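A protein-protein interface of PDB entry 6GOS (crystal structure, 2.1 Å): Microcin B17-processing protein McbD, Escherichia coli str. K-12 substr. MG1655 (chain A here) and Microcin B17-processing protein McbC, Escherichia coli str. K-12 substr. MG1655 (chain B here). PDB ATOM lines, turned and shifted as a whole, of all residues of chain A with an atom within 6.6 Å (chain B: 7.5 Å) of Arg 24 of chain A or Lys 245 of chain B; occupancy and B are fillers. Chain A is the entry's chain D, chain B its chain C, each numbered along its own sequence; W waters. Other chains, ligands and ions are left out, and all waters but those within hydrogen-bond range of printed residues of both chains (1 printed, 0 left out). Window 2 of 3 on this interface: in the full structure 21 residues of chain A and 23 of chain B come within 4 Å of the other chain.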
ATOM      1  N   LYS A  21      30.608  -7.388 -19.861  1.00  0.00           N
ATOM      2  CA  LYS A  21      29.415  -8.001 -20.404  1.00  0.00           C
ATOM      3  C   LYS A  21      28.337  -8.000 -19.296  1.00  0.00           C
ATOM      4  O   LYS A  21      28.654  -8.153 -18.102  1.00  0.00           O
ATOM      5  CB  LYS A  21      29.759  -9.414 -20.914  1.00  0.00           C
ATOM      6  CG  LYS A  21      30.059 -10.381 -19.796  1.00  0.00           C
ATOM      7  CD  LYS A  21      30.927 -11.561 -20.157  1.00  0.00           C
ATOM      8  CE  LYS A  21      30.674 -12.639 -19.119  1.00  0.00           C
ATOM      9  NZ  LYS A  21      31.836 -13.507 -18.891  1.00  0.00           N
ATOM     10  N   LEU A  22      27.081  -7.789 -19.667  1.00  0.00           N
ATOM     11  CA  LEU A  22      26.013  -7.852 -18.699  1.00  0.00           C
ATOM     12  C   LEU A  22      25.761  -9.282 -18.245  1.00  0.00           C
ATOM     13  O   LEU A  22      25.450  -9.496 -17.087  1.00  0.00           O
ATOM     14  CB  LEU A  22      24.715  -7.264 -19.242  1.00  0.00           C
ATOM     15  CG  LEU A  22      24.645  -5.787 -19.620  1.00  0.00           C
ATOM     16  CD1 LEU A  22      23.230  -5.431 -20.050  1.00  0.00           C
ATOM     17  CD2 LEU A  22      25.095  -4.916 -18.471  1.00  0.00           C
ATOM     18  N   ASN A  23      25.919 -10.252 -19.143  1.00  0.00           N
ATOM     19  CA  ASN A  23      25.410 -11.617 -18.932  1.00  0.00           C
ATOM     20  C   ASN A  23      26.526 -12.528 -18.431  1.00  0.00           C
ATOM     21  O   ASN A  23      27.496 -12.774 -19.155  1.00  0.00           O
ATOM     22  CB  ASN A  23      24.836 -12.141 -20.261  1.00  0.00           C
ATOM     23  CG  ASN A  23      24.222 -13.524 -20.159  1.00  0.00           C
ATOM     24  OD1 ASN A  23      24.365 -14.235 -19.156  1.00  0.00           O
ATOM     25  ND2 ASN A  23      23.546 -13.926 -21.228  1.00  0.00           N
ATOM     26  N   ARG A  24      26.373 -13.075 -17.226  1.00  0.00           N
ATOM     27  CA  ARG A  24      27.425 -13.912 -16.639  1.00  0.00           C
ATOM     28  C   ARG A  24      27.630 -15.220 -17.395  1.00  0.00           C
ATOM     29  O   ARG A  24      28.718 -15.811 -17.320  1.00  0.00           O
ATOM     30  CB  ARG A  24      27.152 -14.221 -15.163  1.00  0.00           C
ATOM     31  CG  ARG A  24      26.125 -15.312 -14.900  1.00  0.00           C
ATOM     32  CD  ARG A  24      25.774 -15.344 -13.427  1.00  0.00           C
ATOM     33  NE  ARG A  24      24.830 -16.397 -13.111  1.00  0.00           N
ATOM     34  CZ  ARG A  24      25.149 -17.673 -12.911  1.00  0.00           C
ATOM     35  NH1 ARG A  24      26.413 -18.101 -12.963  1.00  0.00           N
ATOM     36  NH2 ARG A  24      24.176 -18.535 -12.644  1.00  0.00           N
ATOM     37  N   ASN A  25      26.587 -15.652 -18.101  1.00  0.00           N
ATOM     38  CA  ASN A  25      26.620 -16.855 -18.922  1.00  0.00           C
ATOM     39  C   ASN A  25      27.046 -16.671 -20.390  1.00  0.00           C
ATOM     40  O   ASN A  25      26.980 -17.629 -21.151  1.00  0.00           O
ATOM     41  CB  ASN A  25      25.245 -17.549 -18.871  1.00  0.00           C
ATOM     42  CG  ASN A  25      24.932 -18.120 -17.506  1.00  0.00           C
ATOM     43  OD1 ASN A  25      25.752 -18.850 -16.949  1.00  0.00           O
ATOM     44  ND2 ASN A  25      23.753 -17.787 -16.951  1.00  0.00           N
ATOM     45  N   MET A  26      27.433 -15.469 -20.810  1.00  0.00           N
ATOM     46  CA  MET A  26      28.076 -15.312 -22.125  1.00  0.00           C
ATOM     47  C   MET A  26      29.576 -15.461 -21.902  1.00  0.00           C
ATOM     48  O   MET A  26      30.057 -15.176 -20.813  1.00  0.00           O
ATOM     49  CB  MET A  26      27.764 -13.965 -22.790  1.00  0.00           C
ATOM     50  CG  MET A  26      26.416 -13.866 -23.526  1.00  0.00           C
ATOM     51  SD  MET A  26      26.191 -14.994 -24.936  1.00  0.00           S
ATOM     52  CE  MET A  26      24.546 -14.540 -25.508  1.00  0.00           C
ATOM     53  N   PRO A  27      30.324 -15.921 -22.926  1.00  0.00           N
ATOM     54  CA  PRO A  27      31.775 -15.972 -22.800  1.00  0.00           C
ATOM     55  C   PRO A  27      32.398 -14.596 -22.655  1.00  0.00           C
ATOM     56  O   PRO A  27      31.850 -13.607 -23.097  1.00  0.00           O
ATOM     57  CB  PRO A  27      32.234 -16.625 -24.112  1.00  0.00           C
ATOM     58  CG  PRO A  27      31.142 -16.315 -25.058  1.00  0.00           C
ATOM     59  CD  PRO A  27      29.888 -16.413 -24.243  1.00  0.00           C
ATOM     60  N   ASN A 196      27.232 -24.015 -19.535  1.00  0.00           N
ATOM     61  CA  ASN A 196      26.344 -22.845 -19.511  1.00  0.00           C
ATOM     62  C   ASN A 196      26.584 -21.914 -20.692  1.00  0.00           C
ATOM     63  O   ASN A 196      25.638 -21.579 -21.412  1.00  0.00           O
ATOM     64  CB  ASN A 196      26.458 -22.054 -18.182  1.00  0.00           C
ATOM     65  CG  ASN A 196      25.618 -22.654 -17.057  1.00  0.00           C
ATOM     66  OD1 ASN A 196      24.576 -23.268 -17.290  1.00  0.00           O
ATOM     67  ND2 ASN A 196      26.073 -22.467 -15.824  1.00  0.00           N
ATOM     68  N   HIS A 197      27.837 -21.523 -20.904  1.00  0.00           N
ATOM     69  CA  HIS A 197      28.134 -20.525 -21.926  1.00  0.00           C
ATOM     70  C   HIS A 197      27.985 -21.038 -23.370  1.00  0.00           C
ATOM     71  O   HIS A 197      27.679 -20.259 -24.278  1.00  0.00           O
ATOM     72  CB  HIS A 197      29.476 -19.816 -21.665  1.00  0.00           C
ATOM     73  CG  HIS A 197      30.699 -20.618 -22.001  1.00  0.00           C
ATOM     74  ND1 HIS A 197      31.253 -21.535 -21.133  1.00  0.00           N
ATOM     75  CD2 HIS A 197      31.511 -20.588 -23.087  1.00  0.00           C
ATOM     76  CE1 HIS A 197      32.335 -22.058 -21.683  1.00  0.00           C
ATOM     77  NE2 HIS A 197      32.513 -21.503 -22.871  1.00  0.00           N
ATOM     78  N   ALA B 163      16.179 -13.909 -18.130  1.00  0.00           N
ATOM     79  CA  ALA B 163      16.253 -15.175 -17.380  1.00  0.00           C
ATOM     80  C   ALA B 163      14.934 -15.918 -17.195  1.00  0.00           C
ATOM     81  O   ALA B 163      13.871 -15.317 -17.028  1.00  0.00           O
ATOM     82  CB  ALA B 163      16.915 -14.938 -16.029  1.00  0.00           C
ATOM     83  N   CYS B 165      14.537 -18.054 -14.587  1.00  0.00           N
ATOM     84  CA  CYS B 165      14.390 -18.429 -13.193  1.00  0.00           C
ATOM     85  C   CYS B 165      12.915 -18.328 -12.803  1.00  0.00           C
ATOM     86  O   CYS B 165      12.164 -17.536 -13.382  1.00  0.00           O
ATOM     87  CB  CYS B 165      15.236 -17.530 -12.283  1.00  0.00           C
ATOM     88  SG  CYS B 165      14.927 -15.750 -12.437  1.00  0.00           S
ATOM     89  N   SER B 173      15.089 -13.351  -3.645  1.00  0.00           N
ATOM     90  CA  SER B 173      16.319 -12.555  -3.806  1.00  0.00           C
ATOM     91  C   SER B 173      16.063 -11.057  -3.624  1.00  0.00           C
ATOM     92  O   SER B 173      16.790 -10.353  -2.897  1.00  0.00           O
ATOM     93  CB  SER B 173      17.020 -12.853  -5.157  1.00  0.00           C
ATOM     94  OG  SER B 173      16.432 -12.166  -6.270  1.00  0.00           O
ATOM     95  N   THR B 239      19.823  -8.531  -0.820  1.00  0.00           N
ATOM     96  CA  THR B 239      21.183  -8.981  -0.954  1.00  0.00           C
ATOM     97  C   THR B 239      21.646  -8.725  -2.394  1.00  0.00           C
ATOM     98  O   THR B 239      21.239  -9.420  -3.309  1.00  0.00           O
ATOM     99  CB  THR B 239      21.280 -10.472  -0.585  1.00  0.00           C
ATOM    100  OG1 THR B 239      20.762 -10.668   0.735  1.00  0.00           O
ATOM    101  CG2 THR B 239      22.699 -10.961  -0.663  1.00  0.00           C
ATOM    102  N   ASP B 240      22.482  -7.711  -2.580  1.00  0.00           N
ATOM    103  CA  ASP B 240      22.930  -7.299  -3.921  1.00  0.00           C
ATOM    104  C   ASP B 240      23.476  -8.433  -4.797  1.00  0.00           C
ATOM    105  O   ASP B 240      23.043  -8.578  -5.954  1.00  0.00           O
ATOM    106  CB  ASP B 240      23.981  -6.205  -3.855  1.00  0.00           C
ATOM    107  CG  ASP B 240      23.505  -4.989  -3.086  1.00  0.00           C
ATOM    108  OD1 ASP B 240      23.252  -5.135  -1.876  1.00  0.00           O
ATOM    109  OD2 ASP B 240      23.368  -3.905  -3.689  1.00  0.00           O
ATOM    110  N   SER B 241      24.419  -9.206  -4.273  1.00  0.00           N
ATOM    111  CA  SER B 241      25.041 -10.256  -5.070  1.00  0.00           C
ATOM    112  C   SER B 241      24.068 -11.380  -5.456  1.00  0.00           C
ATOM    113  O   SER B 241      24.208 -11.969  -6.525  1.00  0.00           O
ATOM    114  CB  SER B 241      26.279 -10.821  -4.381  1.00  0.00           C
ATOM    115  OG  SER B 241      25.901 -11.368  -3.142  1.00  0.00           O
ATOM    116  N   TYR B 242      23.085 -11.644  -4.594  1.00  0.00           N
ATOM    117  CA  TYR B 242      22.111 -12.710  -4.777  1.00  0.00           C
ATOM    118  C   TYR B 242      21.076 -12.309  -5.834  1.00  0.00           C
ATOM    119  O   TYR B 242      20.684 -13.131  -6.670  1.00  0.00           O
ATOM    120  CB  TYR B 242      21.452 -13.028  -3.428  1.00  0.00           C
ATOM    121  CG  TYR B 242      20.400 -14.128  -3.353  1.00  0.00           C
ATOM    122  CD1 TYR B 242      20.462 -15.277  -4.147  1.00  0.00           C
ATOM    123  CD2 TYR B 242      19.363 -14.040  -2.424  1.00  0.00           C
ATOM    124  CE1 TYR B 242      19.507 -16.275  -4.031  1.00  0.00           C
ATOM    125  CE2 TYR B 242      18.402 -15.025  -2.312  1.00  0.00           C
ATOM    126  CZ  TYR B 242      18.482 -16.135  -3.107  1.00  0.00           C
ATOM    127  OH  TYR B 242      17.534 -17.111  -2.968  1.00  0.00           O
ATOM    128  N   VAL B 243      20.648 -11.057  -5.785  1.00  0.00           N
ATOM    129  CA  VAL B 243      19.841 -10.478  -6.851  1.00  0.00           C
ATOM    130  C   VAL B 243      20.575 -10.566  -8.201  1.00  0.00           C
ATOM    131  O   VAL B 243      20.014 -11.051  -9.181  1.00  0.00           O
ATOM    132  CB  VAL B 243      19.491  -9.013  -6.548  1.00  0.00           C
ATOM    133  CG1 VAL B 243      18.925  -8.324  -7.775  1.00  0.00           C
ATOM    134  CG2 VAL B 243      18.493  -8.964  -5.390  1.00  0.00           C
ATOM    135  N   ALA B 244      21.825 -10.119  -8.223  1.00  0.00           N
ATOM    136  CA  ALA B 244      22.643 -10.192  -9.441  1.00  0.00           C
ATOM    137  C   ALA B 244      22.710 -11.610 -10.031  1.00  0.00           C
ATOM    138  O   ALA B 244      22.406 -11.799 -11.228  1.00  0.00           O
ATOM    139  CB  ALA B 244      24.038  -9.648  -9.193  1.00  0.00           C
ATOM    140  N   LYS B 245      23.054 -12.585  -9.185  1.00  0.00           N
ATOM    141  CA  LYS B 245      23.186 -13.985  -9.580  1.00  0.00           C
ATOM    142  C   LYS B 245      21.865 -14.510 -10.134  1.00  0.00           C
ATOM    143  O   LYS B 245      21.866 -15.226 -11.143  1.00  0.00           O
ATOM    144  CB  LYS B 245      23.606 -14.841  -8.375  1.00  0.00           C
ATOM    145  CG  LYS B 245      23.870 -16.327  -8.621  1.00  0.00           C
ATOM    146  CD  LYS B 245      25.336 -16.603  -8.941  1.00  0.00           C
ATOM    147  N   THR B 246      20.750 -14.143  -9.481  1.00  0.00           N
ATOM    148  CA  THR B 246      19.435 -14.685  -9.811  1.00  0.00           C
ATOM    149  C   THR B 246      19.003 -14.201 -11.204  1.00  0.00           C
ATOM    150  O   THR B 246      18.408 -14.948 -11.986  1.00  0.00           O
ATOM    151  CB  THR B 246      18.379 -14.323  -8.731  1.00  0.00           C
ATOM    152  OG1 THR B 246      18.749 -14.916  -7.466  1.00  0.00           O
ATOM    153  CG2 THR B 246      16.997 -14.871  -9.106  1.00  0.00           C
ATOM    154  N   MET B 247      19.347 -12.947 -11.485  1.00  0.00           N
ATOM    155  CA  MET B 247      19.153 -12.293 -12.780  1.00  0.00           C
ATOM    156  C   MET B 247      20.214 -12.616 -13.857  1.00  0.00           C
ATOM    157  O   MET B 247      20.133 -12.109 -14.995  1.00  0.00           O
ATOM    158  CB  MET B 247      19.110 -10.782 -12.556  1.00  0.00           C
ATOM    159  CG  MET B 247      17.873 -10.329 -11.797  1.00  0.00           C
ATOM    160  SD  MET B 247      17.936  -8.588 -11.331  1.00  0.00           S
ATOM    161  CE  MET B 247      17.887  -7.811 -12.919  1.00  0.00           C
ATOM    162  N   ASN B 248      21.193 -13.446 -13.505  1.00  0.00           N
ATOM    163  CA  ASN B 248      22.317 -13.802 -14.392  1.00  0.00           C
ATOM    164  C   ASN B 248      23.161 -12.613 -14.842  1.00  0.00           C
ATOM    165  O   ASN B 248      23.754 -12.623 -15.918  1.00  0.00           O
ATOM    166  CB  ASN B 248      21.829 -14.655 -15.582  1.00  0.00           C
ATOM    167  CG  ASN B 248      21.404 -16.040 -15.153  1.00  0.00           C
ATOM    168  OD1 ASN B 248      22.087 -16.707 -14.370  1.00  0.00           O
ATOM    169  ND2 ASN B 248      20.272 -16.480 -15.655  1.00  0.00           N
ATOM    170  N   LEU B 249      23.246 -11.603 -13.984  1.00  0.00           N
ATOM    171  CA  LEU B 249      24.138 -10.471 -14.200  1.00  0.00           C
ATOM    172  C   LEU B 249      25.588 -10.812 -13.798  1.00  0.00           C
ATOM    173  O   LEU B 249      25.843 -11.572 -12.858  1.00  0.00           O
ATOM    174  CB  LEU B 249      23.663  -9.263 -13.402  1.00  0.00           C
ATOM    175  CG  LEU B 249      22.256  -8.731 -13.668  1.00  0.00           C
ATOM    176  CD1 LEU B 249      22.008  -7.533 -12.755  1.00  0.00           C
ATOM    177  CD2 LEU B 249      22.085  -8.333 -15.122  1.00  0.00           C
ATOM    178  N   ASP B 250      26.527 -10.218 -14.515  1.00  0.00           N
ATOM    179  CA  ASP B 250      27.922 -10.349 -14.215  1.00  0.00           C
ATOM    180  C   ASP B 250      28.344  -9.198 -13.306  1.00  0.00           C
ATOM    181  O   ASP B 250      28.447  -8.045 -13.744  1.00  0.00           O
ATOM    182  CB  ASP B 250      28.721 -10.354 -15.507  1.00  0.00           C
ATOM    183  CG  ASP B 250      30.156 -10.769 -15.292  1.00  0.00           C
ATOM    184  OD1 ASP B 250      30.729 -10.396 -14.227  1.00  0.00           O
ATOM    185  OD2 ASP B 250      30.725 -11.434 -16.208  1.00  0.00           O
ATOM    186  N   GLN B 251      28.599  -9.526 -12.033  1.00  0.00           N
ATOM    187  CA  GLN B 251      28.943  -8.520 -11.012  1.00  0.00           C
ATOM    188  C   GLN B 251      30.247  -7.774 -11.286  1.00  0.00           C
ATOM    189  O   GLN B 251      30.441  -6.684 -10.783  1.00  0.00           O
ATOM    190  CB  GLN B 251      28.934  -9.145  -9.612  1.00  0.00           C
ATOM    191  CG  GLN B 251      27.531  -9.538  -9.164  1.00  0.00           C
ATOM    192  CD  GLN B 251      27.526 -10.213  -7.820  1.00  0.00           C
ATOM    193  OE1 GLN B 251      27.611  -9.553  -6.806  1.00  0.00           O
ATOM    194  NE2 GLN B 251      27.450 -11.529  -7.811  1.00  0.00           N
ATOM    195  N   ARG B 252      31.108  -8.307 -12.154  1.00  0.00           N
ATOM    196  CA  ARG B 252      32.288  -7.551 -12.602  1.00  0.00           C
ATOM    197  C   ARG B 252      31.957  -6.318 -13.452  1.00  0.00           C
ATOM    198  O   ARG B 252      32.704  -5.344 -13.460  1.00  0.00           O
ATOM    199  CB  ARG B 252      33.276  -8.472 -13.289  1.00  0.00           C
ATOM    200  CG  ARG B 252      33.858  -9.516 -12.335  1.00  0.00           C
ATOM    201  CD  ARG B 252      34.527 -10.685 -13.045  1.00  0.00           C
ATOM    202  NE  ARG B 252      33.615 -11.339 -13.988  1.00  0.00           N
ATOM    203  CZ  ARG B 252      33.967 -12.284 -14.858  1.00  0.00           C
ATOM    204  NH1 ARG B 252      35.208 -12.756 -14.903  1.00  0.00           N
ATOM    205  NH2 ARG B 252      33.061 -12.787 -15.683  1.00  0.00           N
ATOM    206  N   VAL B 254      28.247  -5.098 -13.893  1.00  0.00           N
ATOM    207  CA  VAL B 254      26.962  -4.477 -13.611  1.00  0.00           C
ATOM    208  C   VAL B 254      26.516  -4.822 -12.198  1.00  0.00           C
ATOM    209  O   VAL B 254      26.777  -5.908 -11.732  1.00  0.00           O
ATOM    210  CB  VAL B 254      25.903  -4.864 -14.679  1.00  0.00           C
ATOM    211  CG1 VAL B 254      25.713  -6.377 -14.785  1.00  0.00           C
ATOM    212  CG2 VAL B 254      24.581  -4.171 -14.416  1.00  0.00           C
ATOM    213  N   PRO B 256      23.148  -4.134  -9.215  1.00  0.00           N
ATOM    214  CA  PRO B 256      21.858  -3.565  -8.815  1.00  0.00           C
ATOM    215  C   PRO B 256      22.015  -2.466  -7.760  1.00  0.00           C
ATOM    216  O   PRO B 256      22.539  -2.720  -6.688  1.00  0.00           O
ATOM    217  CB  PRO B 256      21.110  -4.776  -8.240  1.00  0.00           C
ATOM    218  CG  PRO B 256      22.165  -5.717  -7.786  1.00  0.00           C
ATOM    219  CD  PRO B 256      23.366  -5.488  -8.639  1.00  0.00           C
HETATM  220  O   HOH W   1      21.287 -18.009 -11.519  1.00  0.00           O
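OD1 of Asn 248 of chain B is in hydrogen-bond range of ND2 of Asn 25 of chain A, at 3.3 Å.
The backbone carbonyl oxygen of Asn 248 of chain B lies within hydrogen-bond range of the backbone NH of Arg 24 of chain A, 3.0 Å away.
O of Leu 22 of chain A lies within hydrogen-bond range of N of Asp 250 of chain B (2.9 Å).
The side-chain amino group (NZ) of Lys 21 of chain A is in salt-bridge range of the side-chain carboxylate (OD2) of Asp 250 of chain B (3.6 Å).
O of Met 26 of chain A sits at hydrogen-bond distance from NZ of Lys 21 of chain A (3.1 Å).
O of Ala 244 of chain B sits at hydrogen-bond distance from N of Leu 249 of chain B, at 2.9 Å.
OD2 of Asp 250 of chain B is in salt-bridge range of NH2 of Arg 252 of chain B.
OD1 of Asn 23 of chain A sits at hydrogen-bond distance from N of Asn 25 of chain A (2.8 Å).
Arg 252 of chain B touches Lys 21 of chain A (NH2 to NZ, 3.5 Å).
O of Leu 22 of chain A touches O of Asn 248 of chain B, at 3.7 Å.
Leu 22 of chain A touches Leu 249 of chain B (O to CA, 3.3 Å).
CB of Val 254 of chain B touches CD2 of Leu 22 of chain A, 3.9 Å away.
Asn 248 of chain B touches Asn 23 of chain A.
Arg 24 of chain A touches Lys 245 of chain B (NE to O, 3.7 Å).
Leu 249 of chain B touches Arg 24 of chain A (O to CB, 3.7 Å).
Arg 24 of chain A touches Asp 250 of chain B.
Of chain B, only Lys 245, Asn 248, Leu 249 and Asp 250 come within 4 Å of Arg 24 of chain A.
Of the printed residues of chain B, Asn 25 of chain A touches Asn 248 (3.3 Å).
Lys 245 of chain B touches just one residue of chain A: Arg 24.
Printed residues of chain A within 4 Å of Asn 248 of chain B: Leu 22, Asn 23, Arg 24 and Asn 25.
Of the 9 printed residues of chain A, 5 touch a printed residue of chain B.
Hydrophobic or aromatic side chains of chain A that line the printed part of chain B: Leu 22.
Along chain A the printed residues that touch a printed residue of chain B span positions 21 to 25.
Of the 19 printed residues of chain B, 6 touch a printed residue of chain A.
Among the printed residues, 12 pairs touch across the chains.
Among the printed residues, Asp or Glu carboxylates within 4 Å of a Lys or Arg side-chain nitrogen of the other chain: Lys 21 of chain A with Asp 250 of chain B.
Water W1 lies within hydrogen-bond range of the backbone carbonyl oxygen (O) of Lys 245 of chain B (2.9 Å), the guanidinium group (NH2) of Arg 24 of chain A (3.1 Å) and the side-chain amide oxygen (OD1) of Asn 248 of chain B (3.2 Å).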
